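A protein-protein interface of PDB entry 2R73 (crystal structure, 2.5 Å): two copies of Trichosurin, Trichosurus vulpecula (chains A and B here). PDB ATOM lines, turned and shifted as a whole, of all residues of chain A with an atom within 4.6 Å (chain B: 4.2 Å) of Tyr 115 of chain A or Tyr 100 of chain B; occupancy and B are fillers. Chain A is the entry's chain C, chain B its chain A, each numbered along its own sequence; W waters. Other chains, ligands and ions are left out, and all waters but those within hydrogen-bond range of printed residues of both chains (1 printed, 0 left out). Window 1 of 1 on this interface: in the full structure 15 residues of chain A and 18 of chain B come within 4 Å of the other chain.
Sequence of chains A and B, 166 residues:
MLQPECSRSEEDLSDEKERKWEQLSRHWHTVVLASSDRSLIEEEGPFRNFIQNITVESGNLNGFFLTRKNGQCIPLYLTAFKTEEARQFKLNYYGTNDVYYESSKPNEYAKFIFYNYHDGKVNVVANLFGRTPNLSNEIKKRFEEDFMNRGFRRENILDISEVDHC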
ATOM      1  N   ARG A  87     -15.816  15.174  32.142  1.00  0.00           N
ATOM      2  CA  ARG A  87     -15.339  14.385  31.007  1.00  0.00           C
ATOM      3  C   ARG A  87     -13.835  14.112  31.087  1.00  0.00           C
ATOM      4  O   ARG A  87     -13.273  13.466  30.202  1.00  0.00           O
ATOM      5  CB  ARG A  87     -15.636  15.119  29.691  1.00  0.00           C
ATOM      6  CG  ARG A  87     -17.110  15.259  29.335  1.00  0.00           C
ATOM      7  CD  ARG A  87     -17.308  16.275  28.206  1.00  0.00           C
ATOM      8  NE  ARG A  87     -16.353  16.068  27.115  1.00  0.00           N
ATOM      9  CZ  ARG A  87     -15.331  16.877  26.844  1.00  0.00           C
ATOM     10  NH1 ARG A  87     -15.130  17.963  27.579  1.00  0.00           N
ATOM     11  NH2 ARG A  87     -14.492  16.584  25.857  1.00  0.00           N
ATOM     12  N   THR A  96       2.304  10.840  32.542  1.00  0.00           N
ATOM     13  CA  THR A  96       1.021  11.338  33.009  1.00  0.00           C
ATOM     14  C   THR A  96       0.123  11.579  31.807  1.00  0.00           C
ATOM     15  O   THR A  96       0.518  12.256  30.865  1.00  0.00           O
ATOM     16  CB  THR A  96       1.186  12.650  33.781  1.00  0.00           C
ATOM     17  OG1 THR A  96       1.980  12.410  34.946  1.00  0.00           O
ATOM     18  CG2 THR A  96      -0.181  13.203  34.206  1.00  0.00           C
ATOM     19  N   ASN A  97      -1.080  11.019  31.846  1.00  0.00           N
ATOM     20  CA  ASN A  97      -2.037  11.170  30.761  1.00  0.00           C
ATOM     21  C   ASN A  97      -3.290  11.918  31.208  1.00  0.00           C
ATOM     22  O   ASN A  97      -3.993  11.478  32.127  1.00  0.00           O
ATOM     23  CB  ASN A  97      -2.473   9.795  30.251  1.00  0.00           C
ATOM     24  CG  ASN A  97      -1.312   8.934  29.811  1.00  0.00           C
ATOM     25  OD1 ASN A  97      -0.836   9.051  28.683  1.00  0.00           O
ATOM     26  ND2 ASN A  97      -0.842   8.059  30.710  1.00  0.00           N
ATOM     27  N   ASP A  98      -3.567  13.059  30.592  1.00  0.00           N
ATOM     28  CA  ASP A  98      -4.795  13.760  30.932  1.00  0.00           C
ATOM     29  C   ASP A  98      -5.728  13.148  29.909  1.00  0.00           C
ATOM     30  O   ASP A  98      -5.474  13.238  28.705  1.00  0.00           O
ATOM     31  CB  ASP A  98      -4.686  15.270  30.725  1.00  0.00           C
ATOM     32  CG  ASP A  98      -3.727  15.923  31.702  1.00  0.00           C
ATOM     33  OD1 ASP A  98      -3.777  15.580  32.904  1.00  0.00           O
ATOM     34  OD2 ASP A  98      -2.933  16.787  31.267  1.00  0.00           O
ATOM     35  N   TYR A 100      -9.605  12.505  28.153  1.00  0.00           N
ATOM     36  CA  TYR A 100     -10.889  13.120  27.836  1.00  0.00           C
ATOM     37  C   TYR A 100     -11.817  12.177  27.081  1.00  0.00           C
ATOM     38  O   TYR A 100     -11.406  11.493  26.138  1.00  0.00           O
ATOM     39  CB  TYR A 100     -10.686  14.386  27.006  1.00  0.00           C
ATOM     40  CG  TYR A 100     -10.114  15.533  27.797  1.00  0.00           C
ATOM     41  CD1 TYR A 100     -10.917  16.275  28.653  1.00  0.00           C
ATOM     42  CD2 TYR A 100      -8.768  15.864  27.704  1.00  0.00           C
ATOM     43  CE1 TYR A 100     -10.393  17.320  29.393  1.00  0.00           C
ATOM     44  CE2 TYR A 100      -8.236  16.909  28.443  1.00  0.00           C
ATOM     45  CZ  TYR A 100      -9.051  17.632  29.282  1.00  0.00           C
ATOM     46  OH  TYR A 100      -8.527  18.670  30.025  1.00  0.00           O
ATOM     47  N   ILE A 113      -9.322  10.465  24.453  1.00  0.00           N
ATOM     48  CA  ILE A 113      -8.145  11.180  23.999  1.00  0.00           C
ATOM     49  C   ILE A 113      -7.144  11.321  25.137  1.00  0.00           C
ATOM     50  O   ILE A 113      -7.484  11.806  26.210  1.00  0.00           O
ATOM     51  CB  ILE A 113      -8.570  12.549  23.453  1.00  0.00           C
ATOM     52  CG1 ILE A 113      -9.573  12.318  22.315  1.00  0.00           C
ATOM     53  CG2 ILE A 113      -7.355  13.340  22.979  1.00  0.00           C
ATOM     54  CD1 ILE A 113     -10.186  13.558  21.760  1.00  0.00           C
ATOM     55  N   PHE A 114      -5.917  10.866  24.906  1.00  0.00           N
ATOM     56  CA  PHE A 114      -4.879  10.938  25.923  1.00  0.00           C
ATOM     57  C   PHE A 114      -3.839  11.991  25.565  1.00  0.00           C
ATOM     58  O   PHE A 114      -3.267  11.961  24.473  1.00  0.00           O
ATOM     59  CB  PHE A 114      -4.104   9.601  26.074  1.00  0.00           C
ATOM     60  CG  PHE A 114      -4.959   8.376  26.341  1.00  0.00           C
ATOM     61  CD1 PHE A 114      -6.305   8.473  26.643  1.00  0.00           C
ATOM     62  CD2 PHE A 114      -4.379   7.111  26.310  1.00  0.00           C
ATOM     63  CE1 PHE A 114      -7.054   7.337  26.907  1.00  0.00           C
ATOM     64  CE2 PHE A 114      -5.119   5.971  26.572  1.00  0.00           C
ATOM     65  CZ  PHE A 114      -6.462   6.086  26.873  1.00  0.00           C
ATOM     66  N   TYR A 115      -3.591  12.927  26.470  1.00  0.00           N
ATOM     67  CA  TYR A 115      -2.539  13.903  26.232  1.00  0.00           C
ATOM     68  C   TYR A 115      -1.442  13.398  27.169  1.00  0.00           C
ATOM     69  O   TYR A 115      -1.508  13.534  28.387  1.00  0.00           O
ATOM     70  CB  TYR A 115      -3.002  15.320  26.570  1.00  0.00           C
ATOM     71  CG  TYR A 115      -4.056  15.827  25.615  1.00  0.00           C
ATOM     72  CD1 TYR A 115      -5.382  15.950  26.013  1.00  0.00           C
ATOM     73  CD2 TYR A 115      -3.736  16.141  24.296  1.00  0.00           C
ATOM     74  CE1 TYR A 115      -6.365  16.367  25.130  1.00  0.00           C
ATOM     75  CE2 TYR A 115      -4.721  16.565  23.397  1.00  0.00           C
ATOM     76  CZ  TYR A 115      -6.029  16.672  23.824  1.00  0.00           C
ATOM     77  OH  TYR A 115      -7.021  17.063  22.942  1.00  0.00           O
ATOM     78  N   ASN A 116      -0.457  12.759  26.568  1.00  0.00           N
ATOM     79  CA  ASN A 116       0.637  12.146  27.291  1.00  0.00           C
ATOM     80  C   ASN A 116       1.906  12.992  27.446  1.00  0.00           C
ATOM     81  O   ASN A 116       2.441  13.520  26.459  1.00  0.00           O
ATOM     82  CB  ASN A 116       0.951  10.829  26.585  1.00  0.00           C
ATOM     83  CG  ASN A 116       2.108  10.093  27.196  1.00  0.00           C
ATOM     84  OD1 ASN A 116       3.246  10.209  26.728  1.00  0.00           O
ATOM     85  ND2 ASN A 116       1.833   9.328  28.249  1.00  0.00           N
ATOM     86  N   TYR A 117       2.361  13.128  28.694  1.00  0.00           N
ATOM     87  CA  TYR A 117       3.587  13.862  29.018  1.00  0.00           C
ATOM     88  C   TYR A 117       4.596  12.843  29.532  1.00  0.00           C
ATOM     89  O   TYR A 117       4.402  12.252  30.590  1.00  0.00           O
ATOM     90  CB  TYR A 117       3.363  14.904  30.119  1.00  0.00           C
ATOM     91  CG  TYR A 117       2.285  15.913  29.833  1.00  0.00           C
ATOM     92  CD1 TYR A 117       0.960  15.650  30.162  1.00  0.00           C
ATOM     93  CD2 TYR A 117       2.586  17.140  29.257  1.00  0.00           C
ATOM     94  CE1 TYR A 117      -0.030  16.583  29.932  1.00  0.00           C
ATOM     95  CE2 TYR A 117       1.593  18.080  29.021  1.00  0.00           C
ATOM     96  CZ  TYR A 117       0.291  17.793  29.367  1.00  0.00           C
ATOM     97  OH  TYR A 117      -0.696  18.728  29.191  1.00  0.00           O
ATOM     98  N   ASN A 123       2.467  14.219  23.814  1.00  0.00           N
ATOM     99  CA  ASN A 123       1.909  13.517  22.675  1.00  0.00           C
ATOM    100  C   ASN A 123       0.409  13.309  22.849  1.00  0.00           C
ATOM    101  O   ASN A 123      -0.142  13.463  23.947  1.00  0.00           O
ATOM    102  CB  ASN A 123       2.589  12.163  22.471  1.00  0.00           C
ATOM    103  CG  ASN A 123       3.966  12.287  21.831  1.00  0.00           C
ATOM    104  OD1 ASN A 123       4.989  12.149  22.503  1.00  0.00           O
ATOM    105  ND2 ASN A 123       3.996  12.555  20.525  1.00  0.00           N
ATOM    106  N   VAL A 124      -0.253  12.970  21.750  1.00  0.00           N
ATOM    107  CA  VAL A 124      -1.671  12.726  21.796  1.00  0.00           C
ATOM    108  C   VAL A 124      -1.916  11.331  21.284  1.00  0.00           C
ATOM    109  O   VAL A 124      -1.378  10.926  20.254  1.00  0.00           O
ATOM    110  CB  VAL A 124      -2.464  13.708  20.923  1.00  0.00           C
ATOM    111  CG1 VAL A 124      -2.121  13.493  19.470  1.00  0.00           C
ATOM    112  CG2 VAL A 124      -3.953  13.501  21.122  1.00  0.00           C
ATOM    113  N   ARG B  87     -17.665  22.078  28.249  1.00  0.00           N
ATOM    114  CA  ARG B  87     -16.471  22.846  28.568  1.00  0.00           C
ATOM    115  C   ARG B  87     -15.361  22.804  27.530  1.00  0.00           C
ATOM    116  O   ARG B  87     -14.223  23.173  27.819  1.00  0.00           O
ATOM    117  CB  ARG B  87     -15.929  22.413  29.940  1.00  0.00           C
ATOM    118  CG  ARG B  87     -16.916  22.701  31.064  1.00  0.00           C
ATOM    119  CD  ARG B  87     -16.247  22.867  32.417  1.00  0.00           C
ATOM    120  NE  ARG B  87     -17.081  23.641  33.340  1.00  0.00           N
ATOM    121  CZ  ARG B  87     -16.706  24.010  34.564  1.00  0.00           C
ATOM    122  NH1 ARG B  87     -15.503  23.675  35.021  1.00  0.00           N
ATOM    123  NH2 ARG B  87     -17.525  24.722  35.331  1.00  0.00           N
ATOM    124  N   GLN B  88     -15.682  22.367  26.320  1.00  0.00           N
ATOM    125  CA  GLN B  88     -14.667  22.310  25.278  1.00  0.00           C
ATOM    126  C   GLN B  88     -14.971  23.251  24.124  1.00  0.00           C
ATOM    127  O   GLN B  88     -16.109  23.332  23.664  1.00  0.00           O
ATOM    128  CB  GLN B  88     -14.527  20.891  24.734  1.00  0.00           C
ATOM    129  CG  GLN B  88     -13.602  20.813  23.538  1.00  0.00           C
ATOM    130  CD  GLN B  88     -13.302  19.391  23.115  1.00  0.00           C
ATOM    131  OE1 GLN B  88     -12.606  19.161  22.127  1.00  0.00           O
ATOM    132  NE2 GLN B  88     -13.827  18.425  23.864  1.00  0.00           N
ATOM    133  N   ASP B  98      -7.657  22.906  20.576  1.00  0.00           N
ATOM    134  CA  ASP B  98      -8.791  22.319  21.260  1.00  0.00           C
ATOM    135  C   ASP B  98      -8.648  22.949  22.649  1.00  0.00           C
ATOM    136  O   ASP B  98      -7.651  22.743  23.345  1.00  0.00           O
ATOM    137  CB  ASP B  98      -8.686  20.794  21.279  1.00  0.00           C
ATOM    138  CG  ASP B  98      -8.848  20.191  19.890  1.00  0.00           C
ATOM    139  OD1 ASP B  98      -9.821  20.555  19.199  1.00  0.00           O
ATOM    140  OD2 ASP B  98      -8.011  19.360  19.483  1.00  0.00           O
ATOM    141  N   VAL B  99      -9.636  23.758  23.014  1.00  0.00           N
ATOM    142  CA  VAL B  99      -9.637  24.495  24.266  1.00  0.00           C
ATOM    143  C   VAL B  99     -10.557  23.911  25.327  1.00  0.00           C
ATOM    144  O   VAL B  99     -11.719  23.612  25.058  1.00  0.00           O
ATOM    145  CB  VAL B  99     -10.043  25.961  23.998  1.00  0.00           C
ATOM    146  CG1 VAL B  99     -10.000  26.779  25.288  1.00  0.00           C
ATOM    147  CG2 VAL B  99      -9.124  26.554  22.939  1.00  0.00           C
ATOM    148  N   TYR B 100     -10.025  23.751  26.537  1.00  0.00           N
ATOM    149  CA  TYR B 100     -10.802  23.218  27.651  1.00  0.00           C
ATOM    150  C   TYR B 100     -10.830  24.235  28.785  1.00  0.00           C
ATOM    151  O   TYR B 100      -9.801  24.826  29.122  1.00  0.00           O
ATOM    152  CB  TYR B 100     -10.193  21.911  28.167  1.00  0.00           C
ATOM    153  CG  TYR B 100     -10.229  20.764  27.182  1.00  0.00           C
ATOM    154  CD1 TYR B 100     -11.281  19.851  27.174  1.00  0.00           C
ATOM    155  CD2 TYR B 100      -9.207  20.587  26.265  1.00  0.00           C
ATOM    156  CE1 TYR B 100     -11.305  18.789  26.270  1.00  0.00           C
ATOM    157  CE2 TYR B 100      -9.224  19.538  25.365  1.00  0.00           C
ATOM    158  CZ  TYR B 100     -10.268  18.645  25.368  1.00  0.00           C
ATOM    159  OH  TYR B 100     -10.267  17.618  24.450  1.00  0.00           O
ATOM    160  N   TYR B 101     -12.015  24.434  29.361  1.00  0.00           N
ATOM    161  CA  TYR B 101     -12.198  25.357  30.475  1.00  0.00           C
ATOM    162  C   TYR B 101     -12.419  24.606  31.784  1.00  0.00           C
ATOM    163  O   TYR B 101     -13.115  23.594  31.823  1.00  0.00           O
ATOM    164  CB  TYR B 101     -13.401  26.268  30.236  1.00  0.00           C
ATOM    165  CG  TYR B 101     -13.915  26.933  31.504  1.00  0.00           C
ATOM    166  CD1 TYR B 101     -13.220  27.974  32.102  1.00  0.00           C
ATOM    167  CD2 TYR B 101     -15.099  26.512  32.098  1.00  0.00           C
ATOM    168  CE1 TYR B 101     -13.691  28.583  33.254  1.00  0.00           C
ATOM    169  CE2 TYR B 101     -15.580  27.109  33.250  1.00  0.00           C
ATOM    170  CZ  TYR B 101     -14.879  28.148  33.825  1.00  0.00           C
ATOM    171  OH  TYR B 101     -15.382  28.775  34.951  1.00  0.00           O
ATOM    172  N   LYS B 111      -9.472  29.090  34.005  1.00  0.00           N
ATOM    173  CA  LYS B 111      -8.337  28.404  33.417  1.00  0.00           C
ATOM    174  C   LYS B 111      -8.699  27.877  32.021  1.00  0.00           C
ATOM    175  O   LYS B 111      -9.729  27.216  31.847  1.00  0.00           O
ATOM    176  CB  LYS B 111      -7.928  27.250  34.340  1.00  0.00           C
ATOM    177  CG  LYS B 111      -6.448  26.920  34.356  1.00  0.00           C
ATOM    178  CD  LYS B 111      -6.100  25.925  35.481  1.00  0.00           C
ATOM    179  CE  LYS B 111      -6.344  26.535  36.855  1.00  0.00           C
ATOM    180  NZ  LYS B 111      -5.898  25.666  37.986  1.00  0.00           N
ATOM    181  N   PHE B 112      -7.874  28.194  31.023  1.00  0.00           N
ATOM    182  CA  PHE B 112      -8.111  27.702  29.669  1.00  0.00           C
ATOM    183  C   PHE B 112      -6.896  26.936  29.157  1.00  0.00           C
ATOM    184  O   PHE B 112      -5.820  27.502  28.991  1.00  0.00           O
ATOM    185  CB  PHE B 112      -8.423  28.844  28.696  1.00  0.00           C
ATOM    186  CG  PHE B 112      -9.795  29.434  28.866  1.00  0.00           C
ATOM    187  CD1 PHE B 112      -9.983  30.590  29.611  1.00  0.00           C
ATOM    188  CD2 PHE B 112     -10.902  28.818  28.298  1.00  0.00           C
ATOM    189  CE1 PHE B 112     -11.262  31.121  29.786  1.00  0.00           C
ATOM    190  CE2 PHE B 112     -12.174  29.337  28.469  1.00  0.00           C
ATOM    191  CZ  PHE B 112     -12.356  30.490  29.213  1.00  0.00           C
ATOM    192  N   ILE B 113      -7.066  25.642  28.917  1.00  0.00           N
ATOM    193  CA  ILE B 113      -5.971  24.827  28.414  1.00  0.00           C
ATOM    194  C   ILE B 113      -6.097  24.684  26.903  1.00  0.00           C
ATOM    195  O   ILE B 113      -7.126  24.229  26.407  1.00  0.00           O
ATOM    196  CB  ILE B 113      -5.968  23.401  29.025  1.00  0.00           C
ATOM    197  CG1 ILE B 113      -5.514  23.417  30.486  1.00  0.00           C
ATOM    198  CG2 ILE B 113      -4.985  22.545  28.274  1.00  0.00           C
ATOM    199  CD1 ILE B 113      -6.304  24.307  31.375  1.00  0.00           C
ATOM    200  N   TYR B 115      -4.726  22.935  23.432  1.00  0.00           N
ATOM    201  CA  TYR B 115      -3.944  21.843  22.867  1.00  0.00           C
ATOM    202  C   TYR B 115      -3.804  22.272  21.399  1.00  0.00           C
ATOM    203  O   TYR B 115      -4.724  22.138  20.594  1.00  0.00           O
ATOM    204  CB  TYR B 115      -4.667  20.506  23.018  1.00  0.00           C
ATOM    205  CG  TYR B 115      -4.619  19.996  24.445  1.00  0.00           C
ATOM    206  CD1 TYR B 115      -5.705  20.149  25.303  1.00  0.00           C
ATOM    207  CD2 TYR B 115      -3.461  19.412  24.952  1.00  0.00           C
ATOM    208  CE1 TYR B 115      -5.638  19.735  26.627  1.00  0.00           C
ATOM    209  CE2 TYR B 115      -3.381  18.998  26.276  1.00  0.00           C
ATOM    210  CZ  TYR B 115      -4.472  19.162  27.104  1.00  0.00           C
ATOM    211  OH  TYR B 115      -4.390  18.747  28.416  1.00  0.00           O
ATOM    212  N   TYR B 117      -2.151  22.402  17.589  1.00  0.00           N
ATOM    213  CA  TYR B 117      -1.630  21.587  16.483  1.00  0.00           C
ATOM    214  C   TYR B 117      -1.200  22.535  15.365  1.00  0.00           C
ATOM    215  O   TYR B 117      -2.026  23.223  14.771  1.00  0.00           O
ATOM    216  CB  TYR B 117      -2.693  20.633  15.945  1.00  0.00           C
ATOM    217  CG  TYR B 117      -3.188  19.626  16.948  1.00  0.00           C
ATOM    218  CD1 TYR B 117      -4.139  19.971  17.904  1.00  0.00           C
ATOM    219  CD2 TYR B 117      -2.715  18.317  16.930  1.00  0.00           C
ATOM    220  CE1 TYR B 117      -4.609  19.033  18.813  1.00  0.00           C
ATOM    221  CE2 TYR B 117      -3.175  17.376  17.836  1.00  0.00           C
ATOM    222  CZ  TYR B 117      -4.122  17.738  18.772  1.00  0.00           C
ATOM    223  OH  TYR B 117      -4.576  16.798  19.667  1.00  0.00           O
HETATM  224  O   HOH W   1     -12.436  16.207  24.264  1.00  0.00           O
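Hydrophobic or aromatic side chains of chain A that line the printed part of chain B: Tyr 100, Tyr 115, Tyr 117 and Val 124. Of the 11 printed residues of chain B, 4 touch a printed residue of chain A. Hydrophobic or aromatic side chains of chain B that line the printed part of chain A: Tyr 100, Tyr 115 and Tyr 117. Among the printed residues, 9 pairs touch across the chains.
Arg 87 of chain A touches Tyr 100 of chain B, but with the chains exchanged Tyr 100 of chain A does not touch Arg 87 of chain B (7.2 Å). Tyr 100 of chain A touches its own counterpart, Tyr 100 of chain B. Tyr 115 of chain A touches Tyr 100 of chain B, but with the chains exchanged Tyr 100 of chain A does not touch Tyr 115 of chain B (4.2 Å). Tyr 115 of chain A touches Tyr 117 of chain B, and with the chains exchanged Tyr 117 of chain A touches Tyr 115 of chain B. Positions printed for both chains: 87, 98, 100, 113, 115 and 117. Of the 9 pairs that touch across the chains among the printed residues, 4 have their exchanged pair printed and touching as well.
Tyr 115 of chain A touches three residues of chain B. Tyr 100 of chain B touches just these residues of chain A: Arg 87 (3.9 Å), Tyr 100 (3.5 Å) and Tyr 115 (3.6 Å). Of the printed residues of chain A, Gln 88 of chain B touches Arg 87 (2.8 Å). Of the printed residues of chain A, Tyr 117 of chain B touches Tyr 115 and Val 124. Printed residues of chain B within 4 Å of Tyr 117 of chain A: Tyr 115 (3.8 Å). Ile 113 of chain A touches none of the printed residues of chain B. The nearest printed residue of chain A that does not touch Tyr 100 of chain B is Ile 113 of chain A (4.9 Å). The nearest printed residue of chain B that does not touch Arg 87 of chain A is Arg 87 of chain B (4.8 Å).
NE2 of Gln 88 of chain B lies close to NH2 of Arg 87 of chain A.
NH2 of Arg 87 of chain A touches CE1 of Tyr 100 of chain B, at 3.9 Å. Asp 98 of chain A touches Tyr 115 of chain B. Tyr 100 of chain A touches Tyr 100 of chain B. Tyr 115 of chain A touches Tyr 100 of chain B. Tyr 115 of chain B touches Tyr 115 of chain A (CE2 to CG, 3.3 Å). Tyr 117 of chain B touches Tyr 115 of chain A. Tyr 115 of chain B touches Tyr 117 of chain A (OH to OH, 3.8 Å). Tyr 117 of chain B touches Val 124 of chain A (OH to CG2, 3.7 Å).
Water W1 lies within hydrogen-bond range of the side-chain hydroxyl of Tyr 100 of chain B, the guanidinium group of Arg 87 of chain A and the side-chain amide nitrogen of Gln 88 of chain B.
O of Asp 98 of chain B is in hydrogen-bond range of N of Tyr 115 of chain B. O of Tyr 100 of chain B is in hydrogen-bond range of N of Ile 113 of chain B (2.9 Å). The backbone carbonyl oxygen of Thr 96 of chain A lies within hydrogen-bond range of the backbone NH of Tyr 117 of chain A, 3.0 Å away. O of Asp 98 of chain A sits at hydrogen-bond distance from N of Tyr 115 of chain A, at 2.9 Å. The backbone NH (N) of Ile 113 of chain A sits at hydrogen-bond distance from the backbone carbonyl oxygen (O) of Tyr 100 of chain A, at 2.9 Å.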
